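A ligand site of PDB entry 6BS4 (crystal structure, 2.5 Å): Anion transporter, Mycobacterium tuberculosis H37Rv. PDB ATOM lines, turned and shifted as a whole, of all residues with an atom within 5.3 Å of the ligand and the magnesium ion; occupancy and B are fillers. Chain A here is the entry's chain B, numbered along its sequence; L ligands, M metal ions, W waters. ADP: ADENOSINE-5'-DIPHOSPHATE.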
ATOM      1  N   ALA A  27      16.547  15.745   0.416  1.00  0.00           N
ATOM      2  CA  ALA A  27      16.837  14.319   0.541  1.00  0.00           C
ATOM      3  C   ALA A  27      17.298  13.777  -0.824  1.00  0.00           C
ATOM      4  O   ALA A  27      17.210  14.485  -1.833  1.00  0.00           O
ATOM      5  CB  ALA A  27      15.603  13.568   1.029  1.00  0.00           C
ATOM      6  N   GLY A  28      17.818  12.549  -0.841  1.00  0.00           N
ATOM      7  CA  GLY A  28      18.206  11.898  -2.087  1.00  0.00           C
ATOM      8  C   GLY A  28      16.989  11.364  -2.835  1.00  0.00           C
ATOM      9  O   GLY A  28      15.985  10.991  -2.227  1.00  0.00           O
ATOM     10  N   GLY A  29      17.109  11.335  -4.156  1.00  0.00           N
ATOM     11  CA  GLY A  29      16.086  10.812  -5.057  1.00  0.00           C
ATOM     12  C   GLY A  29      14.948  11.759  -5.345  1.00  0.00           C
ATOM     13  O   GLY A  29      13.909  11.316  -5.838  1.00  0.00           O
ATOM     14  N   VAL A  30      15.149  13.074  -5.112  1.00  0.00           N
ATOM     15  CA  VAL A  30      14.105  14.092  -5.328  1.00  0.00           C
ATOM     16  C   VAL A  30      14.276  14.891  -6.633  1.00  0.00           C
ATOM     17  O   VAL A  30      13.351  15.579  -7.051  1.00  0.00           O
ATOM     18  CB  VAL A  30      13.936  15.054  -4.106  1.00  0.00           C
ATOM     19  CG1 VAL A  30      13.616  14.267  -2.841  1.00  0.00           C
ATOM     20  CG2 VAL A  30      15.160  15.941  -3.898  1.00  0.00           C
ATOM     21  N   GLY A  31      15.472  14.813  -7.231  1.00  0.00           N
ATOM     22  CA  GLY A  31      15.838  15.558  -8.425  1.00  0.00           C
ATOM     23  C   GLY A  31      16.898  16.635  -8.191  1.00  0.00           C
ATOM     24  O   GLY A  31      16.999  17.555  -9.006  1.00  0.00           O
ATOM     25  N   LYS A  32      17.745  16.508  -7.138  1.00  0.00           N
ATOM     26  CA  LYS A  32      18.790  17.515  -6.861  1.00  0.00           C
ATOM     27  C   LYS A  32      19.830  17.672  -7.955  1.00  0.00           C
ATOM     28  O   LYS A  32      20.164  18.802  -8.298  1.00  0.00           O
ATOM     29  CB  LYS A  32      19.525  17.266  -5.526  1.00  0.00           C
ATOM     30  CG  LYS A  32      18.659  17.233  -4.292  1.00  0.00           C
ATOM     31  CD  LYS A  32      19.490  17.342  -3.034  1.00  0.00           C
ATOM     32  CE  LYS A  32      20.231  16.081  -2.663  1.00  0.00           C
ATOM     33  NZ  LYS A  32      20.927  16.260  -1.376  1.00  0.00           N
ATOM     34  N   THR A  33      20.382  16.567  -8.480  1.00  0.00           N
ATOM     35  CA  THR A  33      21.441  16.575  -9.497  1.00  0.00           C
ATOM     36  C   THR A  33      20.966  17.177 -10.805  1.00  0.00           C
ATOM     37  O   THR A  33      21.664  18.016 -11.369  1.00  0.00           O
ATOM     38  CB  THR A  33      22.077  15.191  -9.655  1.00  0.00           C
ATOM     39  OG1 THR A  33      22.554  14.783  -8.375  1.00  0.00           O
ATOM     40  CG2 THR A  33      23.228  15.199 -10.627  1.00  0.00           C
ATOM     41  N   THR A  34      19.778  16.787 -11.251  1.00  0.00           N
ATOM     42  CA  THR A  34      19.129  17.282 -12.466  1.00  0.00           C
ATOM     43  C   THR A  34      18.728  18.759 -12.303  1.00  0.00           C
ATOM     44  O   THR A  34      18.961  19.529 -13.219  1.00  0.00           O
ATOM     45  CB  THR A  34      17.987  16.339 -12.907  1.00  0.00           C
ATOM     46  OG1 THR A  34      17.139  16.058 -11.797  1.00  0.00           O
ATOM     47  CG2 THR A  34      18.511  15.045 -13.439  1.00  0.00           C
ATOM     48  N   THR A  35      18.215  19.151 -11.127  1.00  0.00           N
ATOM     49  CA  THR A  35      17.883  20.560 -10.836  1.00  0.00           C
ATOM     50  C   THR A  35      19.163  21.399 -10.920  1.00  0.00           C
ATOM     51  O   THR A  35      19.162  22.411 -11.626  1.00  0.00           O
ATOM     52  CB  THR A  35      17.133  20.715  -9.474  1.00  0.00           C
ATOM     53  OG1 THR A  35      15.912  19.989  -9.550  1.00  0.00           O
ATOM     54  CG2 THR A  35      16.827  22.179  -9.120  1.00  0.00           C
ATOM     55  N   ASP A  56      26.436  12.820  -8.099  1.00  0.00           N
ATOM     56  CA  ASP A  56      26.096  11.509  -8.644  1.00  0.00           C
ATOM     57  C   ASP A  56      25.159  11.586  -9.859  1.00  0.00           C
ATOM     58  O   ASP A  56      24.045  11.070  -9.802  1.00  0.00           O
ATOM     59  CB  ASP A  56      25.497  10.622  -7.527  1.00  0.00           C
ATOM     60  CG  ASP A  56      24.288  11.202  -6.769  1.00  0.00           C
ATOM     61  OD1 ASP A  56      23.985  12.426  -6.960  1.00  0.00           O
ATOM     62  OD2 ASP A  56      23.623  10.446  -6.007  1.00  0.00           O
ATOM     63  N   ASP A 154      25.689  20.726  -6.284  1.00  0.00           N
ATOM     64  CA  ASP A 154      24.824  19.580  -6.050  1.00  0.00           C
ATOM     65  C   ASP A 154      25.294  18.989  -4.679  1.00  0.00           C
ATOM     66  O   ASP A 154      26.462  19.129  -4.308  1.00  0.00           O
ATOM     67  CB  ASP A 154      24.981  18.579  -7.197  1.00  0.00           C
ATOM     68  CG  ASP A 154      24.204  17.313  -7.055  1.00  0.00           C
ATOM     69  OD1 ASP A 154      23.187  17.320  -6.320  1.00  0.00           O
ATOM     70  OD2 ASP A 154      24.593  16.306  -7.666  1.00  0.00           O
ATOM     71  N   THR A 155      24.367  18.402  -3.913  1.00  0.00           N
ATOM     72  CA  THR A 155      24.727  17.856  -2.599  1.00  0.00           C
ATOM     73  C   THR A 155      24.522  16.344  -2.549  1.00  0.00           C
ATOM     74  O   THR A 155      23.629  15.842  -3.267  1.00  0.00           O
ATOM     75  CB  THR A 155      24.024  18.597  -1.457  1.00  0.00           C
ATOM     76  OG1 THR A 155      22.625  18.422  -1.591  1.00  0.00           O
ATOM     77  CG2 THR A 155      24.393  20.062  -1.402  1.00  0.00           C
ATOM     78  N   PRO A 157      23.336  12.458  -1.852  1.00  0.00           N
ATOM     79  CA  PRO A 157      22.039  11.925  -1.392  1.00  0.00           C
ATOM     80  C   PRO A 157      22.127  11.426   0.054  1.00  0.00           C
ATOM     81  O   PRO A 157      23.166  10.928   0.510  1.00  0.00           O
ATOM     82  CB  PRO A 157      21.784  10.765  -2.356  1.00  0.00           C
ATOM     83  CG  PRO A 157      23.148  10.279  -2.702  1.00  0.00           C
ATOM     84  CD  PRO A 157      23.969  11.535  -2.822  1.00  0.00           C
ATOM     85  N   ASN A 283       9.206  19.079  -7.004  1.00  0.00           N
ATOM     86  CA  ASN A 283       9.422  18.311  -8.233  1.00  0.00           C
ATOM     87  C   ASN A 283       8.534  17.074  -8.402  1.00  0.00           C
ATOM     88  O   ASN A 283       8.025  16.527  -7.428  1.00  0.00           O
ATOM     89  CB  ASN A 283      10.921  17.945  -8.291  1.00  0.00           C
ATOM     90  CG  ASN A 283      11.434  17.494  -9.629  1.00  0.00           C
ATOM     91  OD1 ASN A 283      10.954  17.899 -10.676  1.00  0.00           O
ATOM     92  ND2 ASN A 283      12.434  16.621  -9.603  1.00  0.00           N
ATOM     93  N   ARG A 284       8.349  16.630  -9.665  1.00  0.00           N
ATOM     94  CA  ARG A 284       7.583  15.441 -10.080  1.00  0.00           C
ATOM     95  C   ARG A 284       6.098  15.565  -9.793  1.00  0.00           C
ATOM     96  O   ARG A 284       5.489  14.596  -9.330  1.00  0.00           O
ATOM     97  CB  ARG A 284       8.125  14.137  -9.423  1.00  0.00           C
ATOM     98  CG  ARG A 284       9.612  13.846  -9.516  1.00  0.00           C
ATOM     99  CD  ARG A 284      10.111  13.756 -10.915  1.00  0.00           C
ATOM    100  NE  ARG A 284       9.659  12.564 -11.637  1.00  0.00           N
ATOM    101  CZ  ARG A 284      10.322  11.408 -11.680  1.00  0.00           C
ATOM    102  NH1 ARG A 284      11.453  11.255 -11.000  1.00  0.00           N
ATOM    103  NH2 ARG A 284       9.849  10.394 -12.395  1.00  0.00           N
ATOM    104  N   VAL A 353       7.368  21.640 -10.225  1.00  0.00           N
ATOM    105  CA  VAL A 353       7.923  21.106 -11.457  1.00  0.00           C
ATOM    106  C   VAL A 353       7.200  19.794 -11.808  1.00  0.00           C
ATOM    107  O   VAL A 353       7.243  18.843 -11.021  1.00  0.00           O
ATOM    108  CB  VAL A 353       9.467  20.986 -11.450  1.00  0.00           C
ATOM    109  CG1 VAL A 353       9.966  20.280 -12.715  1.00  0.00           C
ATOM    110  CG2 VAL A 353      10.121  22.346 -11.304  1.00  0.00           C
ATOM    111  N   PRO A 354       6.496  19.738 -12.954  1.00  0.00           N
ATOM    112  CA  PRO A 354       5.810  18.490 -13.327  1.00  0.00           C
ATOM    113  C   PRO A 354       6.762  17.346 -13.666  1.00  0.00           C
ATOM    114  O   PRO A 354       7.900  17.585 -14.076  1.00  0.00           O
ATOM    115  CB  PRO A 354       4.978  18.882 -14.564  1.00  0.00           C
ATOM    116  CG  PRO A 354       5.049  20.393 -14.645  1.00  0.00           C
ATOM    117  CD  PRO A 354       6.314  20.774 -13.994  1.00  0.00           C
ATOM    118  N   SER A 355       6.299  16.114 -13.498  1.00  0.00           N
ATOM    119  CA  SER A 355       7.026  14.907 -13.896  1.00  0.00           C
ATOM    120  C   SER A 355       6.983  14.937 -15.434  1.00  0.00           C
ATOM    121  O   SER A 355       5.910  15.035 -16.003  1.00  0.00           O
ATOM    122  CB  SER A 355       6.325  13.660 -13.374  1.00  0.00           C
ATOM    123  OG  SER A 355       7.000  12.486 -13.788  1.00  0.00           O
ATOM    124  N   LEU A 356       8.153  14.978 -16.088  1.00  0.00           N
ATOM    125  CA  LEU A 356       8.297  15.069 -17.541  1.00  0.00           C
ATOM    126  C   LEU A 356       8.171  13.693 -18.201  1.00  0.00           C
ATOM    127  O   LEU A 356       8.704  12.730 -17.645  1.00  0.00           O
ATOM    128  CB  LEU A 356       9.633  15.756 -17.919  1.00  0.00           C
ATOM    129  CG  LEU A 356       9.883  17.178 -17.349  1.00  0.00           C
ATOM    130  CD1 LEU A 356      11.280  17.656 -17.668  1.00  0.00           C
ATOM    131  CD2 LEU A 356       8.883  18.201 -17.901  1.00  0.00           C
ATOM    132  N   PHE A 358       9.692  11.750 -20.076  1.00  0.00           N
ATOM    133  CA  PHE A 358      10.995  11.279 -20.564  1.00  0.00           C
ATOM    134  C   PHE A 358      12.000  11.393 -19.401  1.00  0.00           C
ATOM    135  O   PHE A 358      11.722  12.075 -18.427  1.00  0.00           O
ATOM    136  CB  PHE A 358      11.489  12.130 -21.784  1.00  0.00           C
ATOM    137  CG  PHE A 358      11.304  13.632 -21.654  1.00  0.00           C
ATOM    138  CD1 PHE A 358      12.222  14.415 -20.950  1.00  0.00           C
ATOM    139  CD2 PHE A 358      10.225  14.273 -22.265  1.00  0.00           C
ATOM    140  CE1 PHE A 358      12.050  15.792 -20.835  1.00  0.00           C
ATOM    141  CE2 PHE A 358      10.050  15.651 -22.140  1.00  0.00           C
ATOM    142  CZ  PHE A 358      10.957  16.406 -21.428  1.00  0.00           C
ATOM    143  N   ASP A 359      13.149  10.725 -19.511  1.00  0.00           N
ATOM    144  CA  ASP A 359      14.199  10.759 -18.496  1.00  0.00           C
ATOM    145  C   ASP A 359      15.020  12.037 -18.697  1.00  0.00           C
ATOM    146  O   ASP A 359      15.312  12.418 -19.838  1.00  0.00           O
ATOM    147  CB  ASP A 359      15.101   9.500 -18.627  1.00  0.00           C
ATOM    148  CG  ASP A 359      15.941   9.189 -17.393  1.00  0.00           C
ATOM    149  OD1 ASP A 359      15.363   9.115 -16.273  1.00  0.00           O
ATOM    150  OD2 ASP A 359      17.161   8.997 -17.546  1.00  0.00           O
ATOM    151  N   VAL A 360      15.373  12.733 -17.588  1.00  0.00           N
ATOM    152  CA  VAL A 360      16.164  13.975 -17.677  1.00  0.00           C
ATOM    153  C   VAL A 360      17.641  13.552 -17.718  1.00  0.00           C
ATOM    154  O   VAL A 360      18.330  13.562 -16.698  1.00  0.00           O
ATOM    155  CB  VAL A 360      15.823  15.037 -16.591  1.00  0.00           C
ATOM    156  CG1 VAL A 360      16.562  16.344 -16.866  1.00  0.00           C
ATOM    157  CG2 VAL A 360      14.312  15.283 -16.538  1.00  0.00           C
ATOM    158  N   SER A 361      18.072  13.095 -18.895  1.00  0.00           N
ATOM    159  CA  SER A 361      19.386  12.494 -19.054  1.00  0.00           C
ATOM    160  C   SER A 361      20.162  12.977 -20.295  1.00  0.00           C
ATOM    161  O   SER A 361      21.203  12.407 -20.622  1.00  0.00           O
ATOM    162  CB  SER A 361      19.275  10.973 -19.036  1.00  0.00           C
ATOM    163  OG  SER A 361      18.428  10.465 -20.054  1.00  0.00           O
ATOM    164  N   LEU A 369      13.520  20.752 -18.475  1.00  0.00           N
ATOM    165  CA  LEU A 369      13.455  20.880 -17.015  1.00  0.00           C
ATOM    166  C   LEU A 369      13.638  22.359 -16.583  1.00  0.00           C
ATOM    167  O   LEU A 369      12.805  22.878 -15.850  1.00  0.00           O
ATOM    168  CB  LEU A 369      14.462  19.945 -16.301  1.00  0.00           C
ATOM    169  CG  LEU A 369      14.378  19.942 -14.748  1.00  0.00           C
ATOM    170  CD1 LEU A 369      13.099  19.303 -14.281  1.00  0.00           C
ATOM    171  CD2 LEU A 369      15.523  19.204 -14.153  1.00  0.00           C
HETATM  172  PB  ADP L   1      18.725  13.127  -6.759  1.00  0.00           P
HETATM  173  O1B ADP L   1      17.867  13.988  -5.937  1.00  0.00           O
HETATM  174  O2B ADP L   1      18.959  11.718  -6.195  1.00  0.00           O
HETATM  175  O3B ADP L   1      20.077  13.759  -7.079  1.00  0.00           O
HETATM  176  PA  ADP L   1      18.223  13.061  -9.678  1.00  0.00           P
HETATM  177  O1A ADP L   1      18.422  14.476 -10.056  1.00  0.00           O
HETATM  178  O2A ADP L   1      19.369  12.163 -10.158  1.00  0.00           O
HETATM  179  O3A ADP L   1      17.938  12.887  -8.118  1.00  0.00           O
HETATM  180  O5' ADP L   1      16.863  12.515 -10.282  1.00  0.00           O
HETATM  181  C5' ADP L   1      16.275  11.247  -9.949  1.00  0.00           C
HETATM  182  C4' ADP L   1      15.647  10.704 -11.215  1.00  0.00           C
HETATM  183  O4' ADP L   1      14.443  11.451 -11.483  1.00  0.00           O
HETATM  184  C3' ADP L   1      16.519  10.828 -12.466  1.00  0.00           C
HETATM  185  O3' ADP L   1      16.318   9.686 -13.304  1.00  0.00           O
HETATM  186  C2' ADP L   1      15.969  12.093 -13.146  1.00  0.00           C
HETATM  187  O2' ADP L   1      16.127  11.976 -14.562  1.00  0.00           O
HETATM  188  C1' ADP L   1      14.489  11.990 -12.791  1.00  0.00           C
HETATM  189  N9  ADP L   1      13.783  13.269 -12.768  1.00  0.00           N
HETATM  190  C8  ADP L   1      14.095  14.358 -11.993  1.00  0.00           C
HETATM  191  N7  ADP L   1      13.266  15.369 -12.117  1.00  0.00           N
HETATM  192  C5  ADP L   1      12.340  14.917 -13.044  1.00  0.00           C
HETATM  193  C6  ADP L   1      11.199  15.521 -13.615  1.00  0.00           C
HETATM  194  N6  ADP L   1      10.748  16.740 -13.263  1.00  0.00           N
HETATM  195  N1  ADP L   1      10.504  14.804 -14.530  1.00  0.00           N
HETATM  196  C2  ADP L   1      10.935  13.579 -14.867  1.00  0.00           C
HETATM  197  N3  ADP L   1      11.992  12.903 -14.387  1.00  0.00           N
HETATM  198  C4  ADP L   1      12.647  13.628 -13.458  1.00  0.00           C
HETATM  199 MG    MG M   1      22.010  13.295  -6.864  1.00  0.00          MG
HETATM  200  O   HOH W   1      22.582  14.779  -5.522  1.00  0.00           O
HETATM  201  O   HOH W   2      21.005  12.188 -12.591  1.00  0.00           O
HETATM  202  O   HOH W   3      18.500   9.104 -15.185  1.00  0.00           O
HETATM  203  O   HOH W   4      19.015   9.266  -7.403  1.00  0.00           O
HETATM  204  O   HOH W   5      19.913   9.346 -10.364  1.00  0.00           O
HETATM  205  O   HOH W   6      18.918  11.852 -14.722  1.00  0.00           O
HETATM  206  O   HOH W   7      18.166   7.894 -11.874  1.00  0.00           O
HETATM  207  O   HOH W   8      21.681  11.897  -8.744  1.00  0.00           O
HETATM  208  O   HOH W   9      21.504  12.004  -5.431  1.00  0.00           O
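The side-chain hydroxyl (OG1) of Thr 155 lies within hydrogen-bond range of the side-chain amino group (NZ) of Lys 32, 2.8 Å away.
N of Arg 284 is in hydrogen-bond range of O of Val 353, at 2.8 Å.
OG1 of Thr 33 sits close to OD2 of Asp 154 (2.6 Å).
The backbone carbonyl oxygen (O) of Val 30 is in hydrogen-bond range of the side-chain amide nitrogen (ND2) of Asn 283 (2.9 Å).
OG of Ser 355 is in hydrogen-bond range of NE of Arg 284 (3.4 Å).
OD2 of Asp 359 lies within hydrogen-bond range of OG of Ser 361 (3.2 Å).
The side-chain hydroxyl (OG1) of Thr 34 lies within hydrogen-bond range of the backbone carbonyl oxygen (O) of Gly 31, 3.2 Å away.
The backbone carbonyl oxygen of Gly 31 lies within hydrogen-bond range of the side-chain hydroxyl of Thr 35, at 2.7 Å.
Water W1 lies within hydrogen-bond range of O of Thr 155 (2.7 Å) and OD1 of Asp 154 (2.7 Å).
Water W9 bridges an oxygen (O2B) of the ligand (2.7 Å) and the side-chain carboxylate (OD2) of Asp 56 (2.7 Å).
Water W8 lies within hydrogen-bond range of the backbone carbonyl oxygen (O) of Asp 56 (2.7 Å) and an oxygen (O2A) of the ligand (2.7 Å).
Water W6 bridges the backbone carbonyl oxygen (O) of Val 360 (2.7 Å) and an oxygen (O2') of the ligand (2.8 Å).
Water W3 lies within hydrogen-bond range of OD2 of Asp 359 and O3' of the ligand.
Water W9 binds the magnesium ion, at 2.0 Å.
The magnesium ion is bound by O3B of the ligand, 2.0 Å away.
Water W1 is bound to the magnesium ion, 2.1 Å away.
The side-chain carboxylate (OD1) of Asp 56 is bound to the magnesium ion (2.2 Å).
OG1 of Thr 33 is bound to the magnesium ion, 2.2 Å away.
Water W8 binds the magnesium ion (2.4 Å).
Gly 28 touches the ligand (C to O2B, 3.9 Å).
Val 353 touches the ligand (CG1 to N6, 3.7 Å).
Ser 355 touches the ligand (CA to N1, 3.5 Å).
O of Phe 358 touches C2 of the ligand (3.9 Å).
CD1 of Leu 369 touches N6 of the ligand (3.6 Å).
Of the 24 residues printed, 17 come within 4 Å of the ligand.
Along chain A the residues within 4 Å of the ligand span positions 28 to 369.
The nearest printed residue that does not touch the ligand is Asp 56 (4.1 Å).
Of the 24 residues printed, 2 come within 4 Å of the magnesium ion.
The guanidinium group of Arg 284 is in hydrogen-bond range of an oxygen (O4') of the ligand, 3.0 Å away.
N of Lys 32 is in hydrogen-bond range of O1B of the ligand (2.8 Å).
The backbone NH (N) of Gly 29 is in hydrogen-bond range of an oxygen (O2B) of the ligand (2.8 Å).
An oxygen (O3') of the ligand is in hydrogen-bond range of the side-chain carboxylate (OD1) of Asp 359 (3.2 Å).
OG1 of Thr 34 is in hydrogen-bond range of O1A of the ligand, 2.7 Å away.
O1B of the ligand lies within hydrogen-bond range of N of Val 30, at 3.0 Å.
An oxygen (O1A) of the ligand is in hydrogen-bond range of the backbone NH (N) of Thr 33.
The backbone NH (N) of Val 360 sits at hydrogen-bond distance from an oxygen (O2') of the ligand, at 3.2 Å.
The backbone carbonyl oxygen of Val 360 is in hydrogen-bond range of an oxygen (O2') of the ligand (3.5 Å).
The side-chain amide oxygen of Asn 283 sits at hydrogen-bond distance from a nitrogen (N6) of the ligand (2.8 Å).
The backbone NH (N) of Thr 34 sits at hydrogen-bond distance from an oxygen (O1A) of the ligand (2.9 Å).
The backbone NH (N) of Leu 356 lies within hydrogen-bond range of a nitrogen (N1) of the ligand (2.8 Å).
A nitrogen (N6) of the ligand is in hydrogen-bond range of the backbone carbonyl oxygen (O) of Pro 354, 3.1 Å away.
The backbone NH (N) of Gly 31 sits at hydrogen-bond distance from an oxygen (O1B) of the ligand.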
